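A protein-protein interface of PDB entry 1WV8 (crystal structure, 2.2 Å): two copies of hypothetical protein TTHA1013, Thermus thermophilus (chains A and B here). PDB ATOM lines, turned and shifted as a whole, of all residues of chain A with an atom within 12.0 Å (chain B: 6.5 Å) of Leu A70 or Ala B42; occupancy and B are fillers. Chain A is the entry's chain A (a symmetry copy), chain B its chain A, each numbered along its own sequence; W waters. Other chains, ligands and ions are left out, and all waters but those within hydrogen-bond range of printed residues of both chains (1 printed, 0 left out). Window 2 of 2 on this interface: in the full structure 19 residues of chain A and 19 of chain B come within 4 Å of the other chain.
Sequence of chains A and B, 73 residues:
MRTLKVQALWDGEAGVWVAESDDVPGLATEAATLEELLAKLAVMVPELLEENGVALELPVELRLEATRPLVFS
N of Leu B4 sits at hydrogen-bond distance from O of Glu B61, at 2.9 Å.
No position is printed for both chains.
Of the 12 pairs that touch across the chains among the printed residues, none has its exchanged pair printed and touching as well.
Hydrophobic or aromatic side chains of chain A that line the printed part of chain B: Leu A70 and Phe A72.
Along chain B the printed residues that touch a printed residue of chain A span positions 4 to 62.
Among the printed residues, no Asp or Glu carboxylate lies within 4 Å of a Lys or Arg side-chain nitrogen of the other chain.
Printed residues of chain B within 4 Å of Arg A68: Ala B42 (3.8 Å), Glu B61 (3.5 Å) and Leu B62 (2.6 Å).
Pro A69 touches none of the printed residues of chain B.
Printed residues of chain B within 4 Å of Phe A72: Pro B46 and Val B60.
Leu B4 touches just one residue of chain A: Leu A70 (3.9 Å).
No residue of chain A comes within 4 Å of Ala B39.
No residue of chain A comes within 4 Å of Leu B41.
Of the printed residues of chain A, Ala B42 touches Arg A68 (3.8 Å) and Leu A70 (3.99 Å).
Val B43 touches none of the printed residues of chain A.
Of chain A, only Leu A70 (3.7 Å) comes within 4 Å of Val B45.
Printed residues of chain A within 4 Å of Pro B46: Phe A72.
The nearest printed residue of chain B that does not touch Leu A70 is Leu B62 (4.02 Å).
The nearest printed residue of chain A that does not touch Ala B42 is Val A71 (5.5 Å).
The nearest printed residue of chain B that does not touch Arg A68 is Leu B38 (4.1 Å).
Water W1 bridges the side-chain carboxylate (OE2) of Glu B61 (2.7 Å) and the side-chain hydroxyl (OG1) of Thr A67 (2.7 Å).
Among the printed residues, merely in contact across the chains: Ala A66 with Leu B62 (3.6 Å), Thr A67 with Glu B61 (3.6 Å), Thr A67 with Leu B62 (3.1 Å), Arg A68 with Ala B42 (3.8 Å), Arg A68 with Glu B61 (3.5 Å), Leu A70 with Leu B4 (3.9 Å), Leu A70 with Ala B42 (3.99 Å), Leu A70 with Val B45 (3.7 Å), Phe A72 with Pro B46 (3.5 Å) and Phe A72 with Val B60 (3.8 Å).
The backbone carbonyl oxygen (O) of Arg A68 is in hydrogen-bond range of the backbone NH (N) of Leu B62 (2.6 Å).
O of Val B60 sits at hydrogen-bond distance from N of Leu A70 (2.9 Å).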
ATOM      1  N   TRP A  17      43.796   2.472  -2.469  1.00  0.00           N
ATOM      2  CA  TRP A  17      42.866   2.597  -1.350  1.00  0.00           C
ATOM      3  C   TRP A  17      43.292   3.888  -0.700  1.00  0.00           C
ATOM      4  O   TRP A  17      44.484   4.132  -0.551  1.00  0.00           O
ATOM      5  CB  TRP A  17      43.035   1.446  -0.350  1.00  0.00           C
ATOM      6  CG  TRP A  17      42.458   0.153  -0.814  1.00  0.00           C
ATOM      7  CD1 TRP A  17      43.107  -0.858  -1.481  1.00  0.00           C
ATOM      8  CD2 TRP A  17      41.116  -0.284  -0.624  1.00  0.00           C
ATOM      9  NE1 TRP A  17      42.240  -1.901  -1.707  1.00  0.00           N
ATOM     10  CE2 TRP A  17      41.012  -1.571  -1.191  1.00  0.00           C
ATOM     11  CE3 TRP A  17      39.986   0.289  -0.031  1.00  0.00           C
ATOM     12  CZ2 TRP A  17      39.812  -2.298  -1.174  1.00  0.00           C
ATOM     13  CZ3 TRP A  17      38.801  -0.431  -0.018  1.00  0.00           C
ATOM     14  CH2 TRP A  17      38.725  -1.712  -0.586  1.00  0.00           C
ATOM     15  N   ALA A  66      36.756  -1.100   5.696  1.00  0.00           N
ATOM     16  CA  ALA A  66      36.540  -1.096   4.257  1.00  0.00           C
ATOM     17  C   ALA A  66      35.128  -1.593   4.021  1.00  0.00           C
ATOM     18  O   ALA A  66      34.780  -2.706   4.438  1.00  0.00           O
ATOM     19  CB  ALA A  66      37.543  -2.015   3.555  1.00  0.00           C
ATOM     20  N   THR A  67      34.315  -0.777   3.354  1.00  0.00           N
ATOM     21  CA  THR A  67      32.935  -1.150   3.090  1.00  0.00           C
ATOM     22  C   THR A  67      32.694  -1.608   1.658  1.00  0.00           C
ATOM     23  O   THR A  67      33.294  -1.100   0.706  1.00  0.00           O
ATOM     24  CB  THR A  67      31.971   0.007   3.438  1.00  0.00           C
ATOM     25  OG1 THR A  67      32.166   0.398   4.807  1.00  0.00           O
ATOM     26  CG2 THR A  67      30.524  -0.429   3.255  1.00  0.00           C
ATOM     27  N   ARG A  68      31.810  -2.593   1.529  1.00  0.00           N
ATOM     28  CA  ARG A  68      31.444  -3.168   0.248  1.00  0.00           C
ATOM     29  C   ARG A  68      29.928  -3.303   0.213  1.00  0.00           C
ATOM     30  O   ARG A  68      29.306  -3.776   1.165  1.00  0.00           O
ATOM     31  CB  ARG A  68      32.079  -4.550   0.090  1.00  0.00           C
ATOM     32  CG  ARG A  68      31.862  -5.206  -1.261  1.00  0.00           C
ATOM     33  CD  ARG A  68      33.194  -5.505  -1.941  1.00  0.00           C
ATOM     34  NE  ARG A  68      33.043  -6.528  -2.974  1.00  0.00           N
ATOM     35  CZ  ARG A  68      34.037  -6.981  -3.747  1.00  0.00           C
ATOM     36  NH1 ARG A  68      35.256  -6.465  -3.650  1.00  0.00           N
ATOM     37  NH2 ARG A  68      33.734  -7.739  -4.799  1.00  0.00           N
ATOM     38  N   PRO A  69      29.308  -2.883  -0.889  1.00  0.00           N
ATOM     39  CA  PRO A  69      27.852  -2.991  -0.981  1.00  0.00           C
ATOM     40  C   PRO A  69      27.445  -4.439  -1.273  1.00  0.00           C
ATOM     41  O   PRO A  69      28.089  -5.104  -2.078  1.00  0.00           O
ATOM     42  CB  PRO A  69      27.531  -2.056  -2.136  1.00  0.00           C
ATOM     43  CG  PRO A  69      28.697  -2.310  -3.064  1.00  0.00           C
ATOM     44  CD  PRO A  69      29.883  -2.307  -2.119  1.00  0.00           C
ATOM     45  N   LEU A  70      26.392  -4.928  -0.622  1.00  0.00           N
ATOM     46  CA  LEU A  70      25.929  -6.301  -0.861  1.00  0.00           C
ATOM     47  C   LEU A  70      24.712  -6.402  -1.783  1.00  0.00           C
ATOM     48  O   LEU A  70      23.734  -5.661  -1.623  1.00  0.00           O
ATOM     49  CB  LEU A  70      25.607  -6.995   0.466  1.00  0.00           C
ATOM     50  CG  LEU A  70      26.834  -7.322   1.324  1.00  0.00           C
ATOM     51  CD1 LEU A  70      26.395  -7.990   2.623  1.00  0.00           C
ATOM     52  CD2 LEU A  70      27.781  -8.227   0.529  1.00  0.00           C
ATOM     53  N   VAL A  71      24.777  -7.334  -2.735  1.00  0.00           N
ATOM     54  CA  VAL A  71      23.693  -7.559  -3.692  1.00  0.00           C
ATOM     55  C   VAL A  71      22.914  -8.845  -3.410  1.00  0.00           C
ATOM     56  O   VAL A  71      23.498  -9.919  -3.224  1.00  0.00           O
ATOM     57  CB  VAL A  71      24.231  -7.632  -5.134  1.00  0.00           C
ATOM     58  CG1 VAL A  71      23.073  -7.763  -6.115  1.00  0.00           C
ATOM     59  CG2 VAL A  71      25.052  -6.389  -5.440  1.00  0.00           C
ATOM     60  N   PHE A  72      21.589  -8.727  -3.386  1.00  0.00           N
ATOM     61  CA  PHE A  72      20.703  -9.864  -3.133  1.00  0.00           C
ATOM     62  C   PHE A  72      19.766 -10.084  -4.314  1.00  0.00           C
ATOM     63  O   PHE A  72      19.855 -11.148  -4.964  1.00  0.00           O
ATOM     64  CB  PHE A  72      19.871  -9.608  -1.878  1.00  0.00           C
ATOM     65  CG  PHE A  72      20.696  -9.368  -0.654  1.00  0.00           C
ATOM     66  CD1 PHE A  72      21.346 -10.421  -0.018  1.00  0.00           C
ATOM     67  CD2 PHE A  72      20.833  -8.083  -0.139  1.00  0.00           C
ATOM     68  CE1 PHE A  72      22.128 -10.197   1.113  1.00  0.00           C
ATOM     69  CE2 PHE A  72      21.611  -7.847   0.993  1.00  0.00           C
ATOM     70  CZ  PHE A  72      22.257  -8.906   1.621  1.00  0.00           C
ATOM     71  N   LEU B   4      26.652  -4.627   8.134  1.00  0.00           N
ATOM     72  CA  LEU B   4      27.092  -5.869   8.759  1.00  0.00           C
ATOM     73  C   LEU B   4      28.588  -5.768   9.023  1.00  0.00           C
ATOM     74  O   LEU B   4      29.393  -5.724   8.088  1.00  0.00           O
ATOM     75  CB  LEU B   4      26.825  -7.059   7.840  1.00  0.00           C
ATOM     76  CG  LEU B   4      25.378  -7.375   7.467  1.00  0.00           C
ATOM     77  CD1 LEU B   4      25.318  -8.430   6.385  1.00  0.00           C
ATOM     78  CD2 LEU B   4      24.654  -7.832   8.715  1.00  0.00           C
ATOM     79  N   LEU B  37      39.711 -11.689   0.781  1.00  0.00           N
ATOM     80  CA  LEU B  37      38.761 -11.936   1.855  1.00  0.00           C
ATOM     81  C   LEU B  37      37.479 -11.166   1.532  1.00  0.00           C
ATOM     82  O   LEU B  37      36.370 -11.667   1.748  1.00  0.00           O
ATOM     83  CB  LEU B  37      39.314 -11.440   3.187  1.00  0.00           C
ATOM     84  CG  LEU B  37      39.023 -12.217   4.480  1.00  0.00           C
ATOM     85  CD1 LEU B  37      38.797 -11.200   5.554  1.00  0.00           C
ATOM     86  CD2 LEU B  37      37.805 -13.118   4.376  1.00  0.00           C
ATOM     87  N   LEU B  38      37.631  -9.944   1.020  1.00  0.00           N
ATOM     88  CA  LEU B  38      36.470  -9.121   0.669  1.00  0.00           C
ATOM     89  C   LEU B  38      35.692  -9.791  -0.444  1.00  0.00           C
ATOM     90  O   LEU B  38      34.481  -9.943  -0.356  1.00  0.00           O
ATOM     91  CB  LEU B  38      36.893  -7.730   0.202  1.00  0.00           C
ATOM     92  CG  LEU B  38      36.835  -6.619   1.250  1.00  0.00           C
ATOM     93  CD1 LEU B  38      37.463  -5.355   0.698  1.00  0.00           C
ATOM     94  CD2 LEU B  38      35.392  -6.376   1.659  1.00  0.00           C
ATOM     95  N   ALA B  39      36.404 -10.179  -1.493  1.00  0.00           N
ATOM     96  CA  ALA B  39      35.788 -10.851  -2.625  1.00  0.00           C
ATOM     97  C   ALA B  39      34.967 -12.042  -2.128  1.00  0.00           C
ATOM     98  O   ALA B  39      33.763 -12.136  -2.394  1.00  0.00           O
ATOM     99  CB  ALA B  39      36.864 -11.317  -3.599  1.00  0.00           C
ATOM    100  N   LYS B  40      35.612 -12.943  -1.387  1.00  0.00           N
ATOM    101  CA  LYS B  40      34.916 -14.119  -0.876  1.00  0.00           C
ATOM    102  C   LYS B  40      33.682 -13.744  -0.052  1.00  0.00           C
ATOM    103  O   LYS B  40      32.620 -14.346  -0.212  1.00  0.00           O
ATOM    104  CB  LYS B  40      35.873 -14.980  -0.050  1.00  0.00           C
ATOM    105  CG  LYS B  40      37.060 -15.499  -0.845  1.00  0.00           C
ATOM    106  CD  LYS B  40      37.906 -16.478  -0.046  1.00  0.00           C
ATOM    107  CE  LYS B  40      38.986 -17.102  -0.927  1.00  0.00           C
ATOM    108  NZ  LYS B  40      39.777 -18.152  -0.225  1.00  0.00           N
ATOM    109  N   LEU B  41      33.813 -12.739   0.811  1.00  0.00           N
ATOM    110  CA  LEU B  41      32.702 -12.305   1.654  1.00  0.00           C
ATOM    111  C   LEU B  41      31.487 -11.824   0.857  1.00  0.00           C
ATOM    112  O   LEU B  41      30.345 -12.114   1.212  1.00  0.00           O
ATOM    113  CB  LEU B  41      33.172 -11.194   2.602  1.00  0.00           C
ATOM    114  CG  LEU B  41      33.719 -11.610   3.978  1.00  0.00           C
ATOM    115  CD1 LEU B  41      34.438 -12.920   3.864  1.00  0.00           C
ATOM    116  CD2 LEU B  41      34.654 -10.533   4.529  1.00  0.00           C
ATOM    117  N   ALA B  42      31.748 -11.090  -0.217  1.00  0.00           N
ATOM    118  CA  ALA B  42      30.692 -10.551  -1.066  1.00  0.00           C
ATOM    119  C   ALA B  42      29.755 -11.644  -1.554  1.00  0.00           C
ATOM    120  O   ALA B  42      28.558 -11.420  -1.727  1.00  0.00           O
ATOM    121  CB  ALA B  42      31.304  -9.829  -2.254  1.00  0.00           C
ATOM    122  N   VAL B  43      30.311 -12.830  -1.765  1.00  0.00           N
ATOM    123  CA  VAL B  43      29.534 -13.965  -2.238  1.00  0.00           C
ATOM    124  C   VAL B  43      28.864 -14.722  -1.092  1.00  0.00           C
ATOM    125  O   VAL B  43      27.643 -14.876  -1.064  1.00  0.00           O
ATOM    126  CB  VAL B  43      30.425 -14.950  -3.013  1.00  0.00           C
ATOM    127  CG1 VAL B  43      29.588 -16.085  -3.545  1.00  0.00           C
ATOM    128  CG2 VAL B  43      31.136 -14.235  -4.150  1.00  0.00           C
ATOM    129  N   MET B  44      29.671 -15.182  -0.143  1.00  0.00           N
ATOM    130  CA  MET B  44      29.176 -15.948   0.995  1.00  0.00           C
ATOM    131  C   MET B  44      28.172 -15.297   1.937  1.00  0.00           C
ATOM    132  O   MET B  44      27.194 -15.932   2.326  1.00  0.00           O
ATOM    133  CB  MET B  44      30.347 -16.436   1.833  1.00  0.00           C
ATOM    134  CG  MET B  44      31.160 -17.530   1.200  1.00  0.00           C
ATOM    135  SD  MET B  44      32.430 -18.149   2.501  1.00  0.00           S
ATOM    136  CE  MET B  44      31.193 -18.690   3.899  1.00  0.00           C
ATOM    137  N   VAL B  45      28.418 -14.050   2.325  1.00  0.00           N
ATOM    138  CA  VAL B  45      27.531 -13.363   3.261  1.00  0.00           C
ATOM    139  C   VAL B  45      26.054 -13.307   2.856  1.00  0.00           C
ATOM    140  O   VAL B  45      25.177 -13.556   3.679  1.00  0.00           O
ATOM    141  CB  VAL B  45      28.037 -11.929   3.555  1.00  0.00           C
ATOM    142  CG1 VAL B  45      26.995 -11.155   4.353  1.00  0.00           C
ATOM    143  CG2 VAL B  45      29.337 -12.002   4.352  1.00  0.00           C
ATOM    144  N   PRO B  46      25.756 -12.980   1.589  1.00  0.00           N
ATOM    145  CA  PRO B  46      24.333 -12.936   1.231  1.00  0.00           C
ATOM    146  C   PRO B  46      23.737 -14.322   1.460  1.00  0.00           C
ATOM    147  O   PRO B  46      22.728 -14.478   2.162  1.00  0.00           O
ATOM    148  CB  PRO B  46      24.358 -12.546  -0.247  1.00  0.00           C
ATOM    149  CG  PRO B  46      25.629 -11.742  -0.362  1.00  0.00           C
ATOM    150  CD  PRO B  46      26.595 -12.575   0.451  1.00  0.00           C
ATOM    151  N   GLU B  47      24.398 -15.318   0.872  1.00  0.00           N
ATOM    152  CA  GLU B  47      23.995 -16.717   0.980  1.00  0.00           C
ATOM    153  C   GLU B  47      23.692 -17.123   2.416  1.00  0.00           C
ATOM    154  O   GLU B  47      22.638 -17.694   2.692  1.00  0.00           O
ATOM    155  CB  GLU B  47      25.094 -17.631   0.435  1.00  0.00           C
ATOM    156  CG  GLU B  47      25.574 -17.287  -0.962  1.00  0.00           C
ATOM    157  CD  GLU B  47      26.673 -18.222  -1.447  1.00  0.00           C
ATOM    158  OE1 GLU B  47      27.635 -18.455  -0.683  1.00  0.00           O
ATOM    159  OE2 GLU B  47      26.582 -18.719  -2.590  1.00  0.00           O
ATOM    160  N   LEU B  49      23.005 -15.249   4.921  1.00  0.00           N
ATOM    161  CA  LEU B  49      21.892 -14.466   5.454  1.00  0.00           C
ATOM    162  C   LEU B  49      20.544 -15.025   4.997  1.00  0.00           C
ATOM    163  O   LEU B  49      19.553 -14.955   5.726  1.00  0.00           O
ATOM    164  CB  LEU B  49      22.027 -13.003   5.031  1.00  0.00           C
ATOM    165  CG  LEU B  49      23.147 -12.246   5.741  1.00  0.00           C
ATOM    166  CD1 LEU B  49      23.380 -10.906   5.060  1.00  0.00           C
ATOM    167  CD2 LEU B  49      22.780 -12.054   7.205  1.00  0.00           C
ATOM    168  N   PRO B  59      19.305  -0.837   1.798  1.00  0.00           N
ATOM    169  CA  PRO B  59      20.252  -1.791   1.209  1.00  0.00           C
ATOM    170  C   PRO B  59      21.344  -2.132   2.224  1.00  0.00           C
ATOM    171  O   PRO B  59      21.755  -1.277   3.017  1.00  0.00           O
ATOM    172  CB  PRO B  59      20.788  -1.032   0.004  1.00  0.00           C
ATOM    173  CG  PRO B  59      20.859   0.363   0.524  1.00  0.00           C
ATOM    174  CD  PRO B  59      19.546   0.522   1.280  1.00  0.00           C
ATOM    175  N   VAL B  60      21.812  -3.377   2.200  1.00  0.00           N
ATOM    176  CA  VAL B  60      22.839  -3.813   3.144  1.00  0.00           C
ATOM    177  C   VAL B  60      24.266  -3.669   2.629  1.00  0.00           C
ATOM    178  O   VAL B  60      24.563  -3.999   1.479  1.00  0.00           O
ATOM    179  CB  VAL B  60      22.627  -5.291   3.566  1.00  0.00           C
ATOM    180  CG1 VAL B  60      23.699  -5.706   4.561  1.00  0.00           C
ATOM    181  CG2 VAL B  60      21.250  -5.469   4.182  1.00  0.00           C
ATOM    182  N   GLU B  61      25.145  -3.169   3.495  1.00  0.00           N
ATOM    183  CA  GLU B  61      26.555  -2.998   3.160  1.00  0.00           C
ATOM    184  C   GLU B  61      27.423  -3.779   4.147  1.00  0.00           C
ATOM    185  O   GLU B  61      27.101  -3.899   5.337  1.00  0.00           O
ATOM    186  CB  GLU B  61      26.949  -1.523   3.199  1.00  0.00           C
ATOM    187  CG  GLU B  61      26.629  -0.831   4.513  1.00  0.00           C
ATOM    188  CD  GLU B  61      27.346   0.503   4.670  1.00  0.00           C
ATOM    189  OE1 GLU B  61      27.275   1.338   3.743  1.00  0.00           O
ATOM    190  OE2 GLU B  61      27.975   0.720   5.729  1.00  0.00           O
ATOM    191  N   LEU B  62      28.526  -4.302   3.636  1.00  0.00           N
ATOM    192  CA  LEU B  62      29.474  -5.077   4.428  1.00  0.00           C
ATOM    193  C   LEU B  62      30.659  -4.208   4.885  1.00  0.00           C
ATOM    194  O   LEU B  62      31.346  -3.618   4.052  1.00  0.00           O
ATOM    195  CB  LEU B  62      29.989  -6.237   3.573  1.00  0.00           C
ATOM    196  CG  LEU B  62      31.029  -7.191   4.153  1.00  0.00           C
ATOM    197  CD1 LEU B  62      30.373  -8.078   5.188  1.00  0.00           C
ATOM    198  CD2 LEU B  62      31.617  -8.034   3.030  1.00  0.00           C
HETATM  199  O   HOH W   1      30.411   1.093   6.761  1.00  0.00           O
